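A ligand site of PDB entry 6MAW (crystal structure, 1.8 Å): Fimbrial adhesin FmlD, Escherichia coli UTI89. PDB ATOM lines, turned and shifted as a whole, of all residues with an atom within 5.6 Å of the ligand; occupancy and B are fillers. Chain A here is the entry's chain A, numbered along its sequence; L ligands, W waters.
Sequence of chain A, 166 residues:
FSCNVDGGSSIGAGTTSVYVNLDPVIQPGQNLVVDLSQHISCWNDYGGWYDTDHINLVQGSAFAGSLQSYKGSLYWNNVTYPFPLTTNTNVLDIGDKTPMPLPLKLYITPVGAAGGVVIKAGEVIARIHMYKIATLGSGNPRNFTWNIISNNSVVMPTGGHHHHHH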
ATOM      1  N   PHE A   1      29.521  21.071   3.491  1.00  0.00           N
ATOM      2  CA  PHE A   1      29.008  20.305   2.349  1.00  0.00           C
ATOM      3  C   PHE A   1      28.905  18.830   2.736  1.00  0.00           C
ATOM      4  O   PHE A   1      29.824  18.282   3.316  1.00  0.00           O
ATOM      5  CB  PHE A   1      29.903  20.468   1.126  1.00  0.00           C
ATOM      6  CG  PHE A   1      29.438  19.688  -0.070  1.00  0.00           C
ATOM      7  CD1 PHE A   1      30.064  18.499  -0.425  1.00  0.00           C
ATOM      8  CD2 PHE A   1      28.364  20.131  -0.828  1.00  0.00           C
ATOM      9  CE1 PHE A   1      29.630  17.762  -1.528  1.00  0.00           C
ATOM     10  CE2 PHE A   1      27.902  19.392  -1.929  1.00  0.00           C
ATOM     11  CZ  PHE A   1      28.535  18.215  -2.285  1.00  0.00           C
ATOM     12  N   SER A   2      27.775  18.208   2.424  1.00  0.00           N
ATOM     13  CA  SER A   2      27.572  16.792   2.772  1.00  0.00           C
ATOM     14  C   SER A   2      26.748  16.091   1.709  1.00  0.00           C
ATOM     15  O   SER A   2      25.975  16.739   0.977  1.00  0.00           O
ATOM     16  CB  SER A   2      26.868  16.670   4.125  1.00  0.00           C
ATOM     17  OG  SER A   2      27.523  17.400   5.138  1.00  0.00           O
ATOM     18  N   CYS A   3      26.897  14.775   1.606  1.00  0.00           N
ATOM     19  CA  CYS A   3      26.056  13.975   0.710  1.00  0.00           C
ATOM     20  C   CYS A   3      25.453  12.790   1.442  1.00  0.00           C
ATOM     21  O   CYS A   3      25.933  12.410   2.506  1.00  0.00           O
ATOM     22  CB  CYS A   3      26.857  13.476  -0.489  1.00  0.00           C
ATOM     23  SG  CYS A   3      27.602  14.779  -1.507  1.00  0.00           S
ATOM     24  N   SER A  10      25.233  11.075   6.661  1.00  0.00           N
ATOM     25  CA  SER A  10      26.006  12.094   5.956  1.00  0.00           C
ATOM     26  C   SER A  10      27.406  11.593   5.565  1.00  0.00           C
ATOM     27  O   SER A  10      28.038  10.822   6.283  1.00  0.00           O
ATOM     28  CB  SER A  10      26.122  13.358   6.813  1.00  0.00           C
ATOM     29  OG  SER A  10      26.455  13.025   8.145  1.00  0.00           O
ATOM     30  N   ILE A  11      27.850  12.060   4.397  1.00  0.00           N
ATOM     31  CA  ILE A  11      29.169  11.763   3.871  1.00  0.00           C
ATOM     32  C   ILE A  11      29.873  13.078   3.575  1.00  0.00           C
ATOM     33  O   ILE A  11      29.321  13.911   2.841  1.00  0.00           O
ATOM     34  CB  ILE A  11      29.083  10.929   2.568  1.00  0.00           C
ATOM     35  CG1 ILE A  11      28.204   9.688   2.776  1.00  0.00           C
ATOM     36  CG2 ILE A  11      30.481  10.550   2.073  1.00  0.00           C
ATOM     37  CD1 ILE A  11      27.690   9.084   1.469  1.00  0.00           C
ATOM     38  N   GLY A  12      31.071  13.267   4.112  1.00  0.00           N
ATOM     39  CA  GLY A  12      31.761  14.544   3.976  1.00  0.00           C
ATOM     40  C   GLY A  12      32.964  14.477   3.055  1.00  0.00           C
ATOM     41  O   GLY A  12      33.481  15.506   2.651  1.00  0.00           O
ATOM     42  N   ALA A  13      33.381  13.257   2.728  1.00  0.00           N
ATOM     43  CA  ALA A  13      34.524  12.981   1.864  1.00  0.00           C
ATOM     44  C   ALA A  13      34.685  11.474   1.736  1.00  0.00           C
ATOM     45  O   ALA A  13      34.023  10.694   2.441  1.00  0.00           O
ATOM     46  CB  ALA A  13      35.808  13.607   2.438  1.00  0.00           C
ATOM     47  N   TRP A  43      24.012  18.409  -0.167  1.00  0.00           N
ATOM     48  CA  TRP A  43      23.467  19.676   0.298  1.00  0.00           C
ATOM     49  C   TRP A  43      24.540  20.578   0.873  1.00  0.00           C
ATOM     50  O   TRP A  43      25.671  20.144   1.150  1.00  0.00           O
ATOM     51  CB  TRP A  43      22.387  19.439   1.354  1.00  0.00           C
ATOM     52  CG  TRP A  43      22.876  18.730   2.604  1.00  0.00           C
ATOM     53  CD1 TRP A  43      23.373  19.306   3.740  1.00  0.00           C
ATOM     54  CD2 TRP A  43      22.898  17.317   2.826  1.00  0.00           C
ATOM     55  NE1 TRP A  43      23.700  18.327   4.665  1.00  0.00           N
ATOM     56  CE2 TRP A  43      23.420  17.094   4.118  1.00  0.00           C
ATOM     57  CE3 TRP A  43      22.522  16.204   2.049  1.00  0.00           C
ATOM     58  CZ2 TRP A  43      23.576  15.819   4.656  1.00  0.00           C
ATOM     59  CZ3 TRP A  43      22.686  14.935   2.592  1.00  0.00           C
ATOM     60  CH2 TRP A  43      23.211  14.749   3.880  1.00  0.00           C
ATOM     61  N   ASN A  44      24.178  21.845   1.029  1.00  0.00           N
ATOM     62  CA  ASN A  44      25.007  22.858   1.681  1.00  0.00           C
ATOM     63  C   ASN A  44      24.688  22.894   3.191  1.00  0.00           C
ATOM     64  O   ASN A  44      23.521  22.800   3.573  1.00  0.00           O
ATOM     65  CB  ASN A  44      24.730  24.207   1.016  1.00  0.00           C
ATOM     66  CG  ASN A  44      25.531  25.344   1.601  1.00  0.00           C
ATOM     67  OD1 ASN A  44      25.285  25.764   2.730  1.00  0.00           O
ATOM     68  ND2 ASN A  44      26.444  25.898   0.806  1.00  0.00           N
ATOM     69  N   ASP A  45      25.704  22.972   4.046  1.00  0.00           N
ATOM     70  CA  ASP A  45      25.444  22.771   5.470  1.00  0.00           C
ATOM     71  C   ASP A  45      25.112  24.042   6.233  1.00  0.00           C
ATOM     72  O   ASP A  45      24.820  23.971   7.427  1.00  0.00           O
ATOM     73  CB  ASP A  45      26.642  22.074   6.126  1.00  0.00           C
ATOM     74  CG  ASP A  45      26.643  20.582   5.868  1.00  0.00           C
ATOM     75  OD1 ASP A  45      25.718  19.905   6.378  1.00  0.00           O
ATOM     76  OD2 ASP A  45      27.536  20.073   5.157  1.00  0.00           O
ATOM     77  N   TYR A  46      25.153  25.187   5.543  1.00  0.00           N
ATOM     78  CA  TYR A  46      24.663  26.453   6.091  1.00  0.00           C
ATOM     79  C   TYR A  46      23.271  26.817   5.570  1.00  0.00           C
ATOM     80  O   TYR A  46      22.436  27.333   6.312  1.00  0.00           O
ATOM     81  CB  TYR A  46      25.608  27.612   5.729  1.00  0.00           C
ATOM     82  CG  TYR A  46      26.971  27.540   6.336  1.00  0.00           C
ATOM     83  CD1 TYR A  46      27.152  27.267   7.684  1.00  0.00           C
ATOM     84  CD2 TYR A  46      28.093  27.757   5.545  1.00  0.00           C
ATOM     85  CE1 TYR A  46      28.425  27.208   8.226  1.00  0.00           C
ATOM     86  CE2 TYR A  46      29.352  27.687   6.078  1.00  0.00           C
ATOM     87  CZ  TYR A  46      29.524  27.417   7.415  1.00  0.00           C
ATOM     88  OH  TYR A  46      30.787  27.375   7.933  1.00  0.00           O
ATOM     89  N   TYR A  50      24.788  30.606   1.331  1.00  0.00           N
ATOM     90  CA  TYR A  50      25.931  31.140   2.021  1.00  0.00           C
ATOM     91  C   TYR A  50      27.047  30.098   1.906  1.00  0.00           C
ATOM     92  O   TYR A  50      26.836  28.913   2.169  1.00  0.00           O
ATOM     93  CB  TYR A  50      25.611  31.448   3.496  1.00  0.00           C
ATOM     94  CG  TYR A  50      26.750  32.143   4.190  1.00  0.00           C
ATOM     95  CD1 TYR A  50      27.001  33.486   3.951  1.00  0.00           C
ATOM     96  CD2 TYR A  50      27.586  31.449   5.062  1.00  0.00           C
ATOM     97  CE1 TYR A  50      28.051  34.133   4.556  1.00  0.00           C
ATOM     98  CE2 TYR A  50      28.645  32.104   5.689  1.00  0.00           C
ATOM     99  CZ  TYR A  50      28.866  33.450   5.427  1.00  0.00           C
ATOM    100  OH  TYR A  50      29.914  34.113   6.020  1.00  0.00           O
ATOM    101  N   ASP A  51      28.222  30.573   1.507  1.00  0.00           N
ATOM    102  CA  ASP A  51      29.369  29.716   1.216  1.00  0.00           C
ATOM    103  C   ASP A  51      28.945  28.598   0.268  1.00  0.00           C
ATOM    104  O   ASP A  51      28.973  27.424   0.602  1.00  0.00           O
ATOM    105  CB  ASP A  51      29.957  29.145   2.506  1.00  0.00           C
ATOM    106  CG  ASP A  51      31.388  28.726   2.332  1.00  0.00           C
ATOM    107  OD1 ASP A  51      31.960  28.146   3.286  1.00  0.00           O
ATOM    108  OD2 ASP A  51      31.954  28.971   1.256  1.00  0.00           O
ATOM    109  N   ASP A  53      28.689  25.749  -2.385  1.00  0.00           N
ATOM    110  CA  ASP A  53      29.569  24.663  -2.766  1.00  0.00           C
ATOM    111  C   ASP A  53      29.585  24.514  -4.270  1.00  0.00           C
ATOM    112  O   ASP A  53      28.548  24.627  -4.925  1.00  0.00           O
ATOM    113  CB  ASP A  53      29.112  23.379  -2.082  1.00  0.00           C
ATOM    114  CG  ASP A  53      29.163  23.495  -0.579  1.00  0.00           C
ATOM    115  OD1 ASP A  53      30.290  23.661  -0.059  1.00  0.00           O
ATOM    116  OD2 ASP A  53      28.089  23.467   0.069  1.00  0.00           O
ATOM    117  N   LYS A 132      34.663  18.789  -4.647  1.00  0.00           N
ATOM    118  CA  LYS A 132      33.926  19.897  -4.028  1.00  0.00           C
ATOM    119  C   LYS A 132      34.879  20.978  -3.565  1.00  0.00           C
ATOM    120  O   LYS A 132      35.878  20.676  -2.925  1.00  0.00           O
ATOM    121  CB  LYS A 132      33.102  19.413  -2.821  1.00  0.00           C
ATOM    122  CG  LYS A 132      32.620  20.563  -1.897  1.00  0.00           C
ATOM    123  CD  LYS A 132      33.463  20.722  -0.608  1.00  0.00           C
ATOM    124  CE  LYS A 132      33.142  22.058   0.091  1.00  0.00           C
ATOM    125  NZ  LYS A 132      33.726  22.156   1.473  1.00  0.00           N
ATOM    126  N   ALA A 134      34.216  25.062  -1.813  1.00  0.00           N
ATOM    127  CA  ALA A 134      33.223  26.069  -1.494  1.00  0.00           C
ATOM    128  C   ALA A 134      33.760  27.446  -1.877  1.00  0.00           C
ATOM    129  O   ALA A 134      34.529  27.561  -2.827  1.00  0.00           O
ATOM    130  CB  ALA A 134      32.820  26.029  -0.029  1.00  0.00           C
ATOM    131  N   GLY A 139      37.995  27.360   0.870  1.00  0.00           N
ATOM    132  CA  GLY A 139      36.942  26.598   0.223  1.00  0.00           C
ATOM    133  C   GLY A 139      36.803  25.191   0.774  1.00  0.00           C
ATOM    134  O   GLY A 139      35.874  24.463   0.383  1.00  0.00           O
ATOM    135  N   ASN A 140      37.726  24.813   1.664  1.00  0.00           N
ATOM    136  CA  ASN A 140      37.783  23.465   2.238  1.00  0.00           C
ATOM    137  C   ASN A 140      37.516  22.373   1.220  1.00  0.00           C
ATOM    138  O   ASN A 140      36.530  21.645   1.320  1.00  0.00           O
ATOM    139  CB  ASN A 140      36.790  23.334   3.408  1.00  0.00           C
ATOM    140  CG  ASN A 140      37.094  24.317   4.527  1.00  0.00           C
ATOM    141  OD1 ASN A 140      38.154  24.237   5.155  1.00  0.00           O
ATOM    142  ND2 ASN A 140      36.193  25.247   4.771  1.00  0.00           N
ATOM    143  N   ARG A 142      37.192  19.071  -0.948  1.00  0.00           N
ATOM    144  CA  ARG A 142      37.006  17.677  -0.545  1.00  0.00           C
ATOM    145  C   ARG A 142      36.851  16.790  -1.775  1.00  0.00           C
ATOM    146  O   ARG A 142      36.300  17.201  -2.809  1.00  0.00           O
ATOM    147  CB  ARG A 142      35.783  17.533   0.379  1.00  0.00           C
ATOM    148  CG  ARG A 142      35.877  18.281   1.719  1.00  0.00           C
ATOM    149  CD  ARG A 142      37.029  17.768   2.600  1.00  0.00           C
ATOM    150  NE  ARG A 142      37.100  18.480   3.885  1.00  0.00           N
ATOM    151  CZ  ARG A 142      37.961  19.463   4.154  1.00  0.00           C
ATOM    152  NH1 ARG A 142      38.838  19.885   3.240  1.00  0.00           N
ATOM    153  NH2 ARG A 142      37.950  20.039   5.353  1.00  0.00           N
HETATM  154  C1  LIG L   1      28.160  22.440   9.675  1.00  0.00           C
HETATM  155  C2  LIG L   1      30.634  20.193   7.810  1.00  0.00           C
HETATM  156  C3  LIG L   1      32.783  19.064   7.634  1.00  0.00           C
HETATM  157  C4  LIG L   1      32.270  23.590   4.928  1.00  0.00           C
HETATM  158  O1  LIG L   1      28.262  23.529   2.718  1.00  0.00           O
HETATM  159  C5  LIG L   1      28.677  24.844   3.045  1.00  0.00           C
HETATM  160  C6  LIG L   1      29.918  24.827   3.877  1.00  0.00           C
HETATM  161  O2  LIG L   1      29.811  23.735   4.875  1.00  0.00           O
HETATM  162  C7  LIG L   1      30.985  23.690   5.730  1.00  0.00           C
HETATM  163  O3  LIG L   1      30.901  22.554   6.516  1.00  0.00           O
HETATM  164  C8  LIG L   1      29.957  22.597   7.556  1.00  0.00           C
HETATM  165  C9  LIG L   1      29.221  23.729   7.906  1.00  0.00           C
HETATM  166  C10 LIG L   1      28.322  23.650   8.965  1.00  0.00           C
HETATM  167  C11 LIG L   1      28.889  21.312   9.332  1.00  0.00           C
HETATM  168  C12 LIG L   1      28.674  20.009  10.111  1.00  0.00           C
HETATM  169  F1  LIG L   1      29.838  19.428  10.411  1.00  0.00           F
HETATM  170  F2  LIG L   1      27.961  19.165   9.362  1.00  0.00           F
HETATM  171  F3  LIG L   1      28.013  20.275  11.247  1.00  0.00           F
HETATM  172  C13 LIG L   1      29.794  21.395   8.260  1.00  0.00           C
HETATM  173  C14 LIG L   1      30.008  19.130   7.162  1.00  0.00           C
HETATM  174  C15 LIG L   1      30.780  18.037   6.759  1.00  0.00           C
HETATM  175  N1  LIG L   1      30.149  16.928   6.103  1.00  0.00           N
HETATM  176  S1  LIG L   1      29.898  15.581   7.023  1.00  0.00           S
HETATM  177  O4  LIG L   1      29.230  14.578   6.250  1.00  0.00           O
HETATM  178  C16 LIG L   1      28.936  15.989   8.468  1.00  0.00           C
HETATM  179  O5  LIG L   1      31.146  15.010   7.415  1.00  0.00           O
HETATM  180  C17 LIG L   1      32.157  17.993   6.992  1.00  0.00           C
HETATM  181  C18 LIG L   1      32.012  20.157   8.053  1.00  0.00           C
HETATM  182  N2  LIG L   1      33.360  23.621   5.887  1.00  0.00           N
HETATM  183  C19 LIG L   1      34.262  22.522   6.081  1.00  0.00           C
HETATM  184  C20 LIG L   1      35.359  22.647   7.118  1.00  0.00           C
HETATM  185  O6  LIG L   1      34.157  21.497   5.411  1.00  0.00           O
HETATM  186  C21 LIG L   1      32.378  24.692   3.958  1.00  0.00           C
HETATM  187  O7  LIG L   1      33.607  24.520   3.189  1.00  0.00           O
HETATM  188  C22 LIG L   1      31.202  24.725   3.057  1.00  0.00           C
HETATM  189  O8  LIG L   1      31.176  23.524   2.229  1.00  0.00           O
HETATM  190  O   HOH W   1      34.435  27.244   2.830  1.00  0.00           O
HETATM  191  O   HOH W   2      33.564  26.088   7.253  1.00  0.00           O
HETATM  192  O   HOH W   3      32.575  20.428   3.438  1.00  0.00           O
HETATM  193  O   HOH W   4      33.958  15.399   9.326  1.00  0.00           O
HETATM  194  O   HOH W   5      34.789  16.824   5.009  1.00  0.00           O
HETATM  195  O   HOH W   6      35.637  19.404   6.160  1.00  0.00           O
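Residues that only touch the ligand: Ser 10, Asn 44, Tyr 46, Asp 51, Ala 134 and Gly 139. Hydrophobic or aromatic side chains within 4 Å of the ligand: Phe 1, Tyr 46 and Ala 134. Of the 19 residues printed, 14 come within 4 Å of the ligand. The nearest printed residue that does not touch the ligand is Arg 142 (4.1 Å).
The backbone NH (N) of Phe 1 is in hydrogen-bond range of the side-chain carboxylate (OD2) of Asp 45, 2.8 Å away. OG of Ser 2 lies within hydrogen-bond range of OD2 of Asp 45. The side-chain amide nitrogen of Asn 44 is in hydrogen-bond range of the backbone carbonyl oxygen of Tyr 50, 3.3 Å away. The side-chain amino group of Lys 132 lies within hydrogen-bond range of the backbone carbonyl oxygen of Asn 140 (2.9 Å). OD1 of Asp 45 is in hydrogen-bond range of NE1 of Trp 43. NZ of Lys 132 is in hydrogen-bond range of O of Gly 139 (3.3 Å). The backbone carbonyl oxygen of Asn 140 lies close to the guanidinium group of Arg 142, 3.5 Å away. The side-chain amide nitrogen (ND2) of Asn 44 lies within hydrogen-bond range of the backbone carbonyl oxygen (O) of Asp 51, at 3.0 Å.
O7 of the ligand sits at hydrogen-bond distance from ND2 of Asn 140 (3.1 Å). The backbone NH of Phe 1 is in hydrogen-bond range of an oxygen (O1) of the ligand (2.9 Å). The side-chain hydroxyl (OG) of Ser 2 is in hydrogen-bond range of a nitrogen (N1) of the ligand (2.8 Å). The backbone NH (N) of Ile 11 lies close to an oxygen (O4) of the ligand (3.4 Å). O of Phe 1 lies within hydrogen-bond range of N1 of the ligand (3.1 Å). N of Asp 45 lies within hydrogen-bond range of O1 of the ligand (2.9 Å). O7 of the ligand sits at hydrogen-bond distance from NZ of Lys 132 (2.9 Å). The backbone NH (N) of Gly 12 is in hydrogen-bond range of an oxygen (O4) of the ligand, 3.1 Å away. OD1 of Asp 53 is in hydrogen-bond range of O8 of the ligand, 2.5 Å away.
Water W6 bridges the guanidinium group of Arg 142 (2.5 Å) and an oxygen (O6) of the ligand (2.7 Å). Water W3 lies within hydrogen-bond range of O6 of the ligand (2.7 Å), NZ of Lys 132 (2.9 Å) and N of Phe 1 (3.1 Å). Water W2 lies within hydrogen-bond range of N2 of the ligand (2.8 Å) and OH of Tyr 46 (3.1 Å). Water W1 lies within hydrogen-bond range of the side-chain carboxylate (OD1) of Asp 51 (2.7 Å), an oxygen (O7) of the ligand (2.9 Å) and the side-chain amide nitrogen (ND2) of Asn 140 (3.3 Å). Water W5 bridges the backbone carbonyl oxygen of Gly 12 (3.0 Å) and the guanidinium group of Arg 142 (3.1 Å).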
